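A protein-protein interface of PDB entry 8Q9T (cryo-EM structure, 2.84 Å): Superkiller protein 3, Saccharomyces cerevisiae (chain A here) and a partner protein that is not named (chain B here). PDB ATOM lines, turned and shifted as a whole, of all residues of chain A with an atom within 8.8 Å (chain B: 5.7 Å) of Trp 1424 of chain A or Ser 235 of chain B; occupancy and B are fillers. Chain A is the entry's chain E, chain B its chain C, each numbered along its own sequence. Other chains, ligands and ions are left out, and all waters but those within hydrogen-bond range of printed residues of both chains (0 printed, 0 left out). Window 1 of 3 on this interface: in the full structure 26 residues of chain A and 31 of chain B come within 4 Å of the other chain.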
ATOM      1  N   ALA A1399     -29.098  -4.170 -18.146  1.00  0.00           N
ATOM      2  CA  ALA A1399     -28.490  -5.175 -19.011  1.00  0.00           C
ATOM      3  C   ALA A1399     -27.043  -4.841 -19.349  1.00  0.00           C
ATOM      4  O   ALA A1399     -26.224  -5.751 -19.508  1.00  0.00           O
ATOM      5  CB  ALA A1399     -29.310  -5.336 -20.288  1.00  0.00           C
ATOM      6  N   GLU A1400     -26.708  -3.555 -19.466  1.00  0.00           N
ATOM      7  CA  GLU A1400     -25.337  -3.175 -19.791  1.00  0.00           C
ATOM      8  C   GLU A1400     -24.380  -3.548 -18.665  1.00  0.00           C
ATOM      9  O   GLU A1400     -23.313  -4.130 -18.904  1.00  0.00           O
ATOM     10  CB  GLU A1400     -25.270  -1.678 -20.084  1.00  0.00           C
ATOM     11  CG  GLU A1400     -25.723  -1.298 -21.482  1.00  0.00           C
ATOM     12  CD  GLU A1400     -27.198  -0.941 -21.543  1.00  0.00           C
ATOM     13  OE1 GLU A1400     -27.960  -1.389 -20.661  1.00  0.00           O
ATOM     14  OE2 GLU A1400     -27.596  -0.212 -22.476  1.00  0.00           O
ATOM     15  N   SER A1403     -24.038  -7.361 -18.481  1.00  0.00           N
ATOM     16  CA  SER A1403     -23.177  -7.866 -19.545  1.00  0.00           C
ATOM     17  C   SER A1403     -21.712  -7.575 -19.250  1.00  0.00           C
ATOM     18  O   SER A1403     -20.841  -8.413 -19.512  1.00  0.00           O
ATOM     19  CB  SER A1403     -23.584  -7.264 -20.887  1.00  0.00           C
ATOM     20  OG  SER A1403     -23.082  -5.948 -21.026  1.00  0.00           O
ATOM     21  N   GLY A1418     -22.562 -12.373 -22.272  1.00  0.00           N
ATOM     22  CA  GLY A1418     -22.575 -10.927 -22.146  1.00  0.00           C
ATOM     23  C   GLY A1418     -22.751 -10.220 -23.474  1.00  0.00           C
ATOM     24  O   GLY A1418     -23.396  -9.173 -23.547  1.00  0.00           O
ATOM     25  N   MET A1419     -22.170 -10.772 -24.543  1.00  0.00           N
ATOM     26  CA  MET A1419     -22.374 -10.194 -25.867  1.00  0.00           C
ATOM     27  C   MET A1419     -23.790 -10.432 -26.371  1.00  0.00           C
ATOM     28  O   MET A1419     -24.334  -9.597 -27.100  1.00  0.00           O
ATOM     29  CB  MET A1419     -21.360 -10.756 -26.859  1.00  0.00           C
ATOM     30  CG  MET A1419     -21.276  -9.962 -28.146  1.00  0.00           C
ATOM     31  SD  MET A1419     -19.845 -10.389 -29.145  1.00  0.00           S
ATOM     32  CE  MET A1419     -20.471 -10.041 -30.782  1.00  0.00           C
ATOM     33  N   PHE A1420     -24.394 -11.564 -26.012  1.00  0.00           N
ATOM     34  CA  PHE A1420     -25.793 -11.786 -26.359  1.00  0.00           C
ATOM     35  C   PHE A1420     -26.696 -10.780 -25.660  1.00  0.00           C
ATOM     36  O   PHE A1420     -27.643 -10.263 -26.262  1.00  0.00           O
ATOM     37  CB  PHE A1420     -26.204 -13.212 -26.000  1.00  0.00           C
ATOM     38  CG  PHE A1420     -27.503 -13.639 -26.612  1.00  0.00           C
ATOM     39  CD1 PHE A1420     -27.558 -14.079 -27.920  1.00  0.00           C
ATOM     40  CD2 PHE A1420     -28.674 -13.598 -25.877  1.00  0.00           C
ATOM     41  CE1 PHE A1420     -28.752 -14.471 -28.482  1.00  0.00           C
ATOM     42  CE2 PHE A1420     -29.872 -13.991 -26.436  1.00  0.00           C
ATOM     43  CZ  PHE A1420     -29.909 -14.428 -27.738  1.00  0.00           C
ATOM     44  N   LEU A1421     -26.420 -10.488 -24.387  1.00  0.00           N
ATOM     45  CA  LEU A1421     -27.245  -9.535 -23.653  1.00  0.00           C
ATOM     46  C   LEU A1421     -27.110  -8.112 -24.177  1.00  0.00           C
ATOM     47  O   LEU A1421     -28.018  -7.302 -23.966  1.00  0.00           O
ATOM     48  CB  LEU A1421     -26.895  -9.560 -22.166  1.00  0.00           C
ATOM     49  CG  LEU A1421     -27.598 -10.610 -21.306  1.00  0.00           C
ATOM     50  CD1 LEU A1421     -27.130 -10.505 -19.867  1.00  0.00           C
ATOM     51  CD2 LEU A1421     -29.104 -10.466 -21.393  1.00  0.00           C
ATOM     52  N   CYS A1422     -26.009  -7.785 -24.846  1.00  0.00           N
ATOM     53  CA  CYS A1422     -25.762  -6.413 -25.270  1.00  0.00           C
ATOM     54  C   CYS A1422     -24.758  -6.385 -26.417  1.00  0.00           C
ATOM     55  O   CYS A1422     -23.582  -6.069 -26.204  1.00  0.00           O
ATOM     56  CB  CYS A1422     -25.254  -5.584 -24.088  1.00  0.00           C
ATOM     57  SG  CYS A1422     -25.437  -3.802 -24.256  1.00  0.00           S
ATOM     58  N   PRO A1423     -25.181  -6.707 -27.644  1.00  0.00           N
ATOM     59  CA  PRO A1423     -24.223  -6.765 -28.761  1.00  0.00           C
ATOM     60  C   PRO A1423     -23.611  -5.426 -29.133  1.00  0.00           C
ATOM     61  O   PRO A1423     -22.597  -5.413 -29.840  1.00  0.00           O
ATOM     62  CB  PRO A1423     -25.059  -7.333 -29.914  1.00  0.00           C
ATOM     63  CG  PRO A1423     -26.467  -7.076 -29.537  1.00  0.00           C
ATOM     64  CD  PRO A1423     -26.525  -7.145 -28.049  1.00  0.00           C
ATOM     65  N   TRP A1424     -24.185  -4.306 -28.700  1.00  0.00           N
ATOM     66  CA  TRP A1424     -23.627  -2.991 -28.985  1.00  0.00           C
ATOM     67  C   TRP A1424     -22.622  -2.541 -27.930  1.00  0.00           C
ATOM     68  O   TRP A1424     -22.318  -1.347 -27.844  1.00  0.00           O
ATOM     69  CB  TRP A1424     -24.746  -1.958 -29.125  1.00  0.00           C
ATOM     70  CG  TRP A1424     -25.688  -1.926 -27.971  1.00  0.00           C
ATOM     71  CD1 TRP A1424     -25.608  -1.127 -26.871  1.00  0.00           C
ATOM     72  CD2 TRP A1424     -26.860  -2.728 -27.800  1.00  0.00           C
ATOM     73  NE1 TRP A1424     -26.656  -1.383 -26.024  1.00  0.00           N
ATOM     74  CE2 TRP A1424     -27.439  -2.362 -26.572  1.00  0.00           C
ATOM     75  CE3 TRP A1424     -27.476  -3.720 -28.566  1.00  0.00           C
ATOM     76  CZ2 TRP A1424     -28.604  -2.953 -26.092  1.00  0.00           C
ATOM     77  CZ3 TRP A1424     -28.630  -4.305 -28.088  1.00  0.00           C
ATOM     78  CH2 TRP A1424     -29.181  -3.920 -26.863  1.00  0.00           C
ATOM     79  N   ASN A1425     -22.107  -3.468 -27.129  1.00  0.00           N
ATOM     80  CA  ASN A1425     -21.098  -3.167 -26.121  1.00  0.00           C
ATOM     81  C   ASN A1425     -19.717  -3.406 -26.718  1.00  0.00           C
ATOM     82  O   ASN A1425     -19.415  -4.516 -27.167  1.00  0.00           O
ATOM     83  CB  ASN A1425     -21.309  -4.033 -24.881  1.00  0.00           C
ATOM     84  CG  ASN A1425     -20.566  -3.512 -23.673  1.00  0.00           C
ATOM     85  OD1 ASN A1425     -19.979  -2.434 -23.709  1.00  0.00           O
ATOM     86  ND2 ASN A1425     -20.585  -4.280 -22.591  1.00  0.00           N
ATOM     87  N   VAL A1426     -18.885  -2.365 -26.722  1.00  0.00           N
ATOM     88  CA  VAL A1426     -17.574  -2.454 -27.361  1.00  0.00           C
ATOM     89  C   VAL A1426     -16.692  -3.471 -26.647  1.00  0.00           C
ATOM     90  O   VAL A1426     -15.974  -4.250 -27.288  1.00  0.00           O
ATOM     91  CB  VAL A1426     -16.916  -1.063 -27.406  1.00  0.00           C
ATOM     92  CG1 VAL A1426     -15.488  -1.161 -27.908  1.00  0.00           C
ATOM     93  CG2 VAL A1426     -17.727  -0.124 -28.278  1.00  0.00           C
ATOM     94  N   THR A1427     -16.728  -3.479 -25.314  1.00  0.00           N
ATOM     95  CA  THR A1427     -15.837  -4.347 -24.550  1.00  0.00           C
ATOM     96  C   THR A1427     -16.150  -5.821 -24.782  1.00  0.00           C
ATOM     97  O   THR A1427     -15.235  -6.645 -24.868  1.00  0.00           O
ATOM     98  CB  THR A1427     -15.922  -4.005 -23.064  1.00  0.00           C
ATOM     99  OG1 THR A1427     -15.819  -2.587 -22.897  1.00  0.00           O
ATOM    100  CG2 THR A1427     -14.795  -4.675 -22.301  1.00  0.00           C
ATOM    101  N   ALA A1428     -17.434  -6.175 -24.879  1.00  0.00           N
ATOM    102  CA  ALA A1428     -17.797  -7.569 -25.122  1.00  0.00           C
ATOM    103  C   ALA A1428     -17.290  -8.048 -26.477  1.00  0.00           C
ATOM    104  O   ALA A1428     -16.739  -9.150 -26.591  1.00  0.00           O
ATOM    105  CB  ALA A1428     -19.313  -7.738 -25.031  1.00  0.00           C
ATOM    106  N   VAL A1429     -17.470  -7.232 -27.517  1.00  0.00           N
ATOM    107  CA  VAL A1429     -16.988  -7.592 -28.845  1.00  0.00           C
ATOM    108  C   VAL A1429     -15.471  -7.710 -28.847  1.00  0.00           C
ATOM    109  O   VAL A1429     -14.903  -8.638 -29.438  1.00  0.00           O
ATOM    110  CB  VAL A1429     -17.482  -6.568 -29.884  1.00  0.00           C
ATOM    111  CG1 VAL A1429     -17.135  -7.022 -31.282  1.00  0.00           C
ATOM    112  CG2 VAL A1429     -18.980  -6.370 -29.752  1.00  0.00           C
ATOM    113  N   PHE B 188     -28.656  -0.152 -33.553  1.00  0.00           N
ATOM    114  CA  PHE B 188     -28.563  -1.595 -33.722  1.00  0.00           C
ATOM    115  C   PHE B 188     -29.943  -2.194 -33.963  1.00  0.00           C
ATOM    116  O   PHE B 188     -30.881  -1.940 -33.203  1.00  0.00           O
ATOM    117  CB  PHE B 188     -27.925  -2.219 -32.482  1.00  0.00           C
ATOM    118  CG  PHE B 188     -27.248  -3.532 -32.737  1.00  0.00           C
ATOM    119  CD1 PHE B 188     -27.958  -4.716 -32.677  1.00  0.00           C
ATOM    120  CD2 PHE B 188     -25.896  -3.585 -33.017  1.00  0.00           C
ATOM    121  CE1 PHE B 188     -27.339  -5.921 -32.902  1.00  0.00           C
ATOM    122  CE2 PHE B 188     -25.273  -4.791 -33.244  1.00  0.00           C
ATOM    123  CZ  PHE B 188     -25.996  -5.959 -33.187  1.00  0.00           C
ATOM    124  N   THR B 190     -32.160  -5.317 -33.698  1.00  0.00           N
ATOM    125  CA  THR B 190     -32.079  -6.483 -32.833  1.00  0.00           C
ATOM    126  C   THR B 190     -33.083  -7.579 -33.151  1.00  0.00           C
ATOM    127  O   THR B 190     -32.853  -8.728 -32.767  1.00  0.00           O
ATOM    128  CB  THR B 190     -32.262  -6.068 -31.365  1.00  0.00           C
ATOM    129  OG1 THR B 190     -33.610  -5.635 -31.155  1.00  0.00           O
ATOM    130  CG2 THR B 190     -31.317  -4.940 -31.009  1.00  0.00           C
ATOM    131  N   PHE B 204     -35.325  -2.010 -32.636  1.00  0.00           N
ATOM    132  CA  PHE B 204     -34.025  -1.388 -32.449  1.00  0.00           C
ATOM    133  C   PHE B 204     -33.684  -1.328 -30.965  1.00  0.00           C
ATOM    134  O   PHE B 204     -34.503  -1.647 -30.102  1.00  0.00           O
ATOM    135  CB  PHE B 204     -33.991   0.012 -33.073  1.00  0.00           C
ATOM    136  CG  PHE B 204     -34.150   0.008 -34.566  1.00  0.00           C
ATOM    137  CD1 PHE B 204     -35.408   0.021 -35.143  1.00  0.00           C
ATOM    138  CD2 PHE B 204     -33.043  -0.022 -35.392  1.00  0.00           C
ATOM    139  CE1 PHE B 204     -35.554   0.011 -36.510  1.00  0.00           C
ATOM    140  CE2 PHE B 204     -33.185  -0.032 -36.759  1.00  0.00           C
ATOM    141  CZ  PHE B 204     -34.442  -0.016 -37.319  1.00  0.00           C
ATOM    142  N   ASN B 205     -32.455  -0.908 -30.676  1.00  0.00           N
ATOM    143  CA  ASN B 205     -31.926  -0.934 -29.318  1.00  0.00           C
ATOM    144  C   ASN B 205     -32.251   0.320 -28.517  1.00  0.00           C
ATOM    145  O   ASN B 205     -31.800   0.436 -27.374  1.00  0.00           O
ATOM    146  CB  ASN B 205     -30.410  -1.145 -29.343  1.00  0.00           C
ATOM    147  CG  ASN B 205     -29.660   0.078 -29.812  1.00  0.00           C
ATOM    148  OD1 ASN B 205     -30.103   0.781 -30.713  1.00  0.00           O
ATOM    149  ND2 ASN B 205     -28.514   0.339 -29.202  1.00  0.00           N
ATOM    150  N   ASN B 206     -32.998   1.265 -29.081  1.00  0.00           N
ATOM    151  CA  ASN B 206     -33.473   2.417 -28.329  1.00  0.00           C
ATOM    152  C   ASN B 206     -34.958   2.344 -28.010  1.00  0.00           C
ATOM    153  O   ASN B 206     -35.495   3.279 -27.412  1.00  0.00           O
ATOM    154  CB  ASN B 206     -33.168   3.715 -29.084  1.00  0.00           C
ATOM    155  CG  ASN B 206     -33.841   3.779 -30.435  1.00  0.00           C
ATOM    156  OD1 ASN B 206     -34.450   2.814 -30.888  1.00  0.00           O
ATOM    157  ND2 ASN B 206     -33.743   4.928 -31.085  1.00  0.00           N
ATOM    158  N   GLY B 207     -35.631   1.263 -28.386  1.00  0.00           N
ATOM    159  CA  GLY B 207     -37.048   1.117 -28.140  1.00  0.00           C
ATOM    160  C   GLY B 207     -37.955   1.497 -29.287  1.00  0.00           C
ATOM    161  O   GLY B 207     -39.168   1.600 -29.081  1.00  0.00           O
ATOM    162  N   SER B 233     -31.633   2.629 -20.836  1.00  0.00           N
ATOM    163  CA  SER B 233     -31.847   1.190 -20.676  1.00  0.00           C
ATOM    164  C   SER B 233     -33.217   0.760 -21.191  1.00  0.00           C
ATOM    165  O   SER B 233     -33.992   0.106 -20.498  1.00  0.00           O
ATOM    166  CB  SER B 233     -31.662   0.799 -19.216  1.00  0.00           C
ATOM    167  N   ASN B 234     -33.521   1.137 -22.430  1.00  0.00           N
ATOM    168  CA  ASN B 234     -34.691   0.661 -23.154  1.00  0.00           C
ATOM    169  C   ASN B 234     -34.208  -0.017 -24.424  1.00  0.00           C
ATOM    170  O   ASN B 234     -33.318   0.502 -25.104  1.00  0.00           O
ATOM    171  CB  ASN B 234     -35.645   1.806 -23.512  1.00  0.00           C
ATOM    172  CG  ASN B 234     -35.769   2.833 -22.409  1.00  0.00           C
ATOM    173  OD1 ASN B 234     -36.186   2.520 -21.296  1.00  0.00           O
ATOM    174  ND2 ASN B 234     -35.403   4.071 -22.713  1.00  0.00           N
ATOM    175  N   SER B 235     -34.785  -1.171 -24.748  1.00  0.00           N
ATOM    176  CA  SER B 235     -34.328  -1.912 -25.916  1.00  0.00           C
ATOM    177  C   SER B 235     -35.357  -2.966 -26.283  1.00  0.00           C
ATOM    178  O   SER B 235     -35.847  -3.685 -25.409  1.00  0.00           O
ATOM    179  CB  SER B 235     -32.968  -2.564 -25.651  1.00  0.00           C
ATOM    180  OG  SER B 235     -32.566  -3.370 -26.741  1.00  0.00           O
ATOM    181  N   ILE B 236     -35.671  -3.060 -27.571  1.00  0.00           N
ATOM    182  CA  ILE B 236     -36.613  -4.059 -28.062  1.00  0.00           C
ATOM    183  C   ILE B 236     -35.905  -5.402 -28.144  1.00  0.00           C
ATOM    184  O   ILE B 236     -34.819  -5.511 -28.722  1.00  0.00           O
ATOM    185  CB  ILE B 236     -37.179  -3.650 -29.429  1.00  0.00           C
ATOM    186  CG1 ILE B 236     -37.742  -2.232 -29.375  1.00  0.00           C
ATOM    187  CG2 ILE B 236     -38.244  -4.632 -29.876  1.00  0.00           C
ATOM    188  CD1 ILE B 236     -38.916  -2.082 -28.460  1.00  0.00           C
ATOM    189  N   ARG B 237     -36.520  -6.431 -27.566  1.00  0.00           N
ATOM    190  CA  ARG B 237     -35.953  -7.771 -27.580  1.00  0.00           C
ATOM    191  C   ARG B 237     -36.689  -8.739 -28.489  1.00  0.00           C
ATOM    192  O   ARG B 237     -36.078  -9.693 -28.969  1.00  0.00           O
ATOM    193  CB  ARG B 237     -35.923  -8.350 -26.162  1.00  0.00           C
ATOM    194  CG  ARG B 237     -35.087  -7.547 -25.192  1.00  0.00           C
ATOM    195  CD  ARG B 237     -34.202  -8.434 -24.342  1.00  0.00           C
ATOM    196  NE  ARG B 237     -33.259  -7.652 -23.555  1.00  0.00           N
ATOM    197  CZ  ARG B 237     -31.946  -7.644 -23.742  1.00  0.00           C
ATOM    198  NH1 ARG B 237     -31.377  -8.391 -24.673  1.00  0.00           N
ATOM    199  NH2 ARG B 237     -31.186  -6.867 -22.979  1.00  0.00           N
ATOM    200  N   ALA B 251     -41.783  -6.929 -26.896  1.00  0.00           N
ATOM    201  CA  ALA B 251     -41.120  -7.126 -25.615  1.00  0.00           C
ATOM    202  C   ALA B 251     -39.912  -6.206 -25.543  1.00  0.00           C
ATOM    203  O   ALA B 251     -39.078  -6.204 -26.452  1.00  0.00           O
ATOM    204  CB  ALA B 251     -40.691  -8.582 -25.432  1.00  0.00           C
ATOM    205  N   HIS B 252     -39.818  -5.425 -24.470  1.00  0.00           N
ATOM    206  CA  HIS B 252     -38.756  -4.441 -24.335  1.00  0.00           C
ATOM    207  C   HIS B 252     -38.333  -4.331 -22.879  1.00  0.00           C
ATOM    208  O   HIS B 252     -39.032  -4.780 -21.969  1.00  0.00           O
ATOM    209  CB  HIS B 252     -39.183  -3.070 -24.879  1.00  0.00           C
ATOM    210  CG  HIS B 252     -40.492  -2.580 -24.343  1.00  0.00           C
ATOM    211  ND1 HIS B 252     -40.580  -1.602 -23.378  1.00  0.00           N
ATOM    212  CD2 HIS B 252     -41.765  -2.922 -24.648  1.00  0.00           C
ATOM    213  CE1 HIS B 252     -41.850  -1.368 -23.105  1.00  0.00           C
ATOM    214  NE2 HIS B 252     -42.590  -2.157 -23.862  1.00  0.00           N
ATOM    215  N   ASP B 253     -37.157  -3.744 -22.673  1.00  0.00           N
ATOM    216  CA  ASP B 253     -36.601  -3.534 -21.345  1.00  0.00           C
ATOM    217  C   ASP B 253     -37.117  -2.236 -20.745  1.00  0.00           C
ATOM    218  O   ASP B 253     -37.422  -1.276 -21.458  1.00  0.00           O
ATOM    219  CB  ASP B 253     -35.074  -3.482 -21.394  1.00  0.00           C
ATOM    220  CG  ASP B 253     -34.453  -4.800 -21.778  1.00  0.00           C
ATOM    221  OD1 ASP B 253     -35.179  -5.812 -21.836  1.00  0.00           O
ATOM    222  OD2 ASP B 253     -33.231  -4.822 -22.027  1.00  0.00           O
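The guanidinium group (NH2) of Arg 237 of chain B sits at hydrogen-bond distance from the backbone carbonyl oxygen (O) of Leu 1421 of chain A (3.3 Å).
The side-chain sulfur of Cys 1422 of chain A sits at hydrogen-bond distance from the indole nitrogen of Trp 1424 of chain A (3.2 Å).
The backbone carbonyl oxygen (O) of Ser 235 of chain B lies within hydrogen-bond range of the backbone NH (N) of Asp 253 of chain B.
The backbone NH (N) of Asn 205 of chain B sits at hydrogen-bond distance from the backbone carbonyl oxygen (O) of Phe 188 of chain B (3.2 Å).
The backbone carbonyl oxygen (O) of Ala 1399 of chain A sits close to the side-chain hydroxyl (OG) of Ser 1403 of chain A.
The guanidinium group (NH2) of Arg 237 of chain B lies within salt-bridge range of the side-chain carboxylate (OD2) of Asp 253 of chain B (3.0 Å).
The backbone carbonyl oxygen of Asn 205 of chain B lies close to the backbone carbonyl oxygen of Asn 234 of chain B (2.7 Å).
Among the printed residues, pairs that only touch across the chains: Trp 1424 of chain A with Ser 235 of chain B, Ala 1399 of chain A with Arg 237 of chain B, Pro 1423 of chain A with Phe 188 of chain B and Trp 1424 of chain A with Asn 205 of chain B.
Of the 15 printed residues of chain A, 4 touch a printed residue of chain B.
Printed residues of chain A that touch a printed residue of chain B: Ala 1399, Leu 1421, Pro 1423 and Trp 1424.
Of the 14 printed residues of chain B, 4 touch a printed residue of chain A.
Hydrophobic or aromatic side chains of chain B within 4 Å of the printed part of chain A: Phe 188.
Of the printed residues of chain B, Trp 1424 of chain A touches Asn 205 and Ser 235.
Ser 235 of chain B touches one residue of chain A.
Printed residues of chain B within 4 Å of Leu 1421 of chain A: Arg 237 (3.3 Å).
Of the printed residues of chain A, Arg 237 of chain B touches Ala 1399 (3.6 Å) and Leu 1421 (3.3 Å).
Of the printed residues of chain B, Pro 1423 of chain A touches Phe 188.
Of the printed residues of chain B, Ala 1399 of chain A touches Arg 237 (3.6 Å).
Asn 1425 of chain A touches none of the printed residues of chain B.
The nearest printed residue of chain B that does not touch Trp 1424 of chain A is Thr 190 of chain B (4.02 Å).
The nearest printed residue of chain B that does not touch Pro 1423 of chain A is Thr 190 of chain B (5.5 Å).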
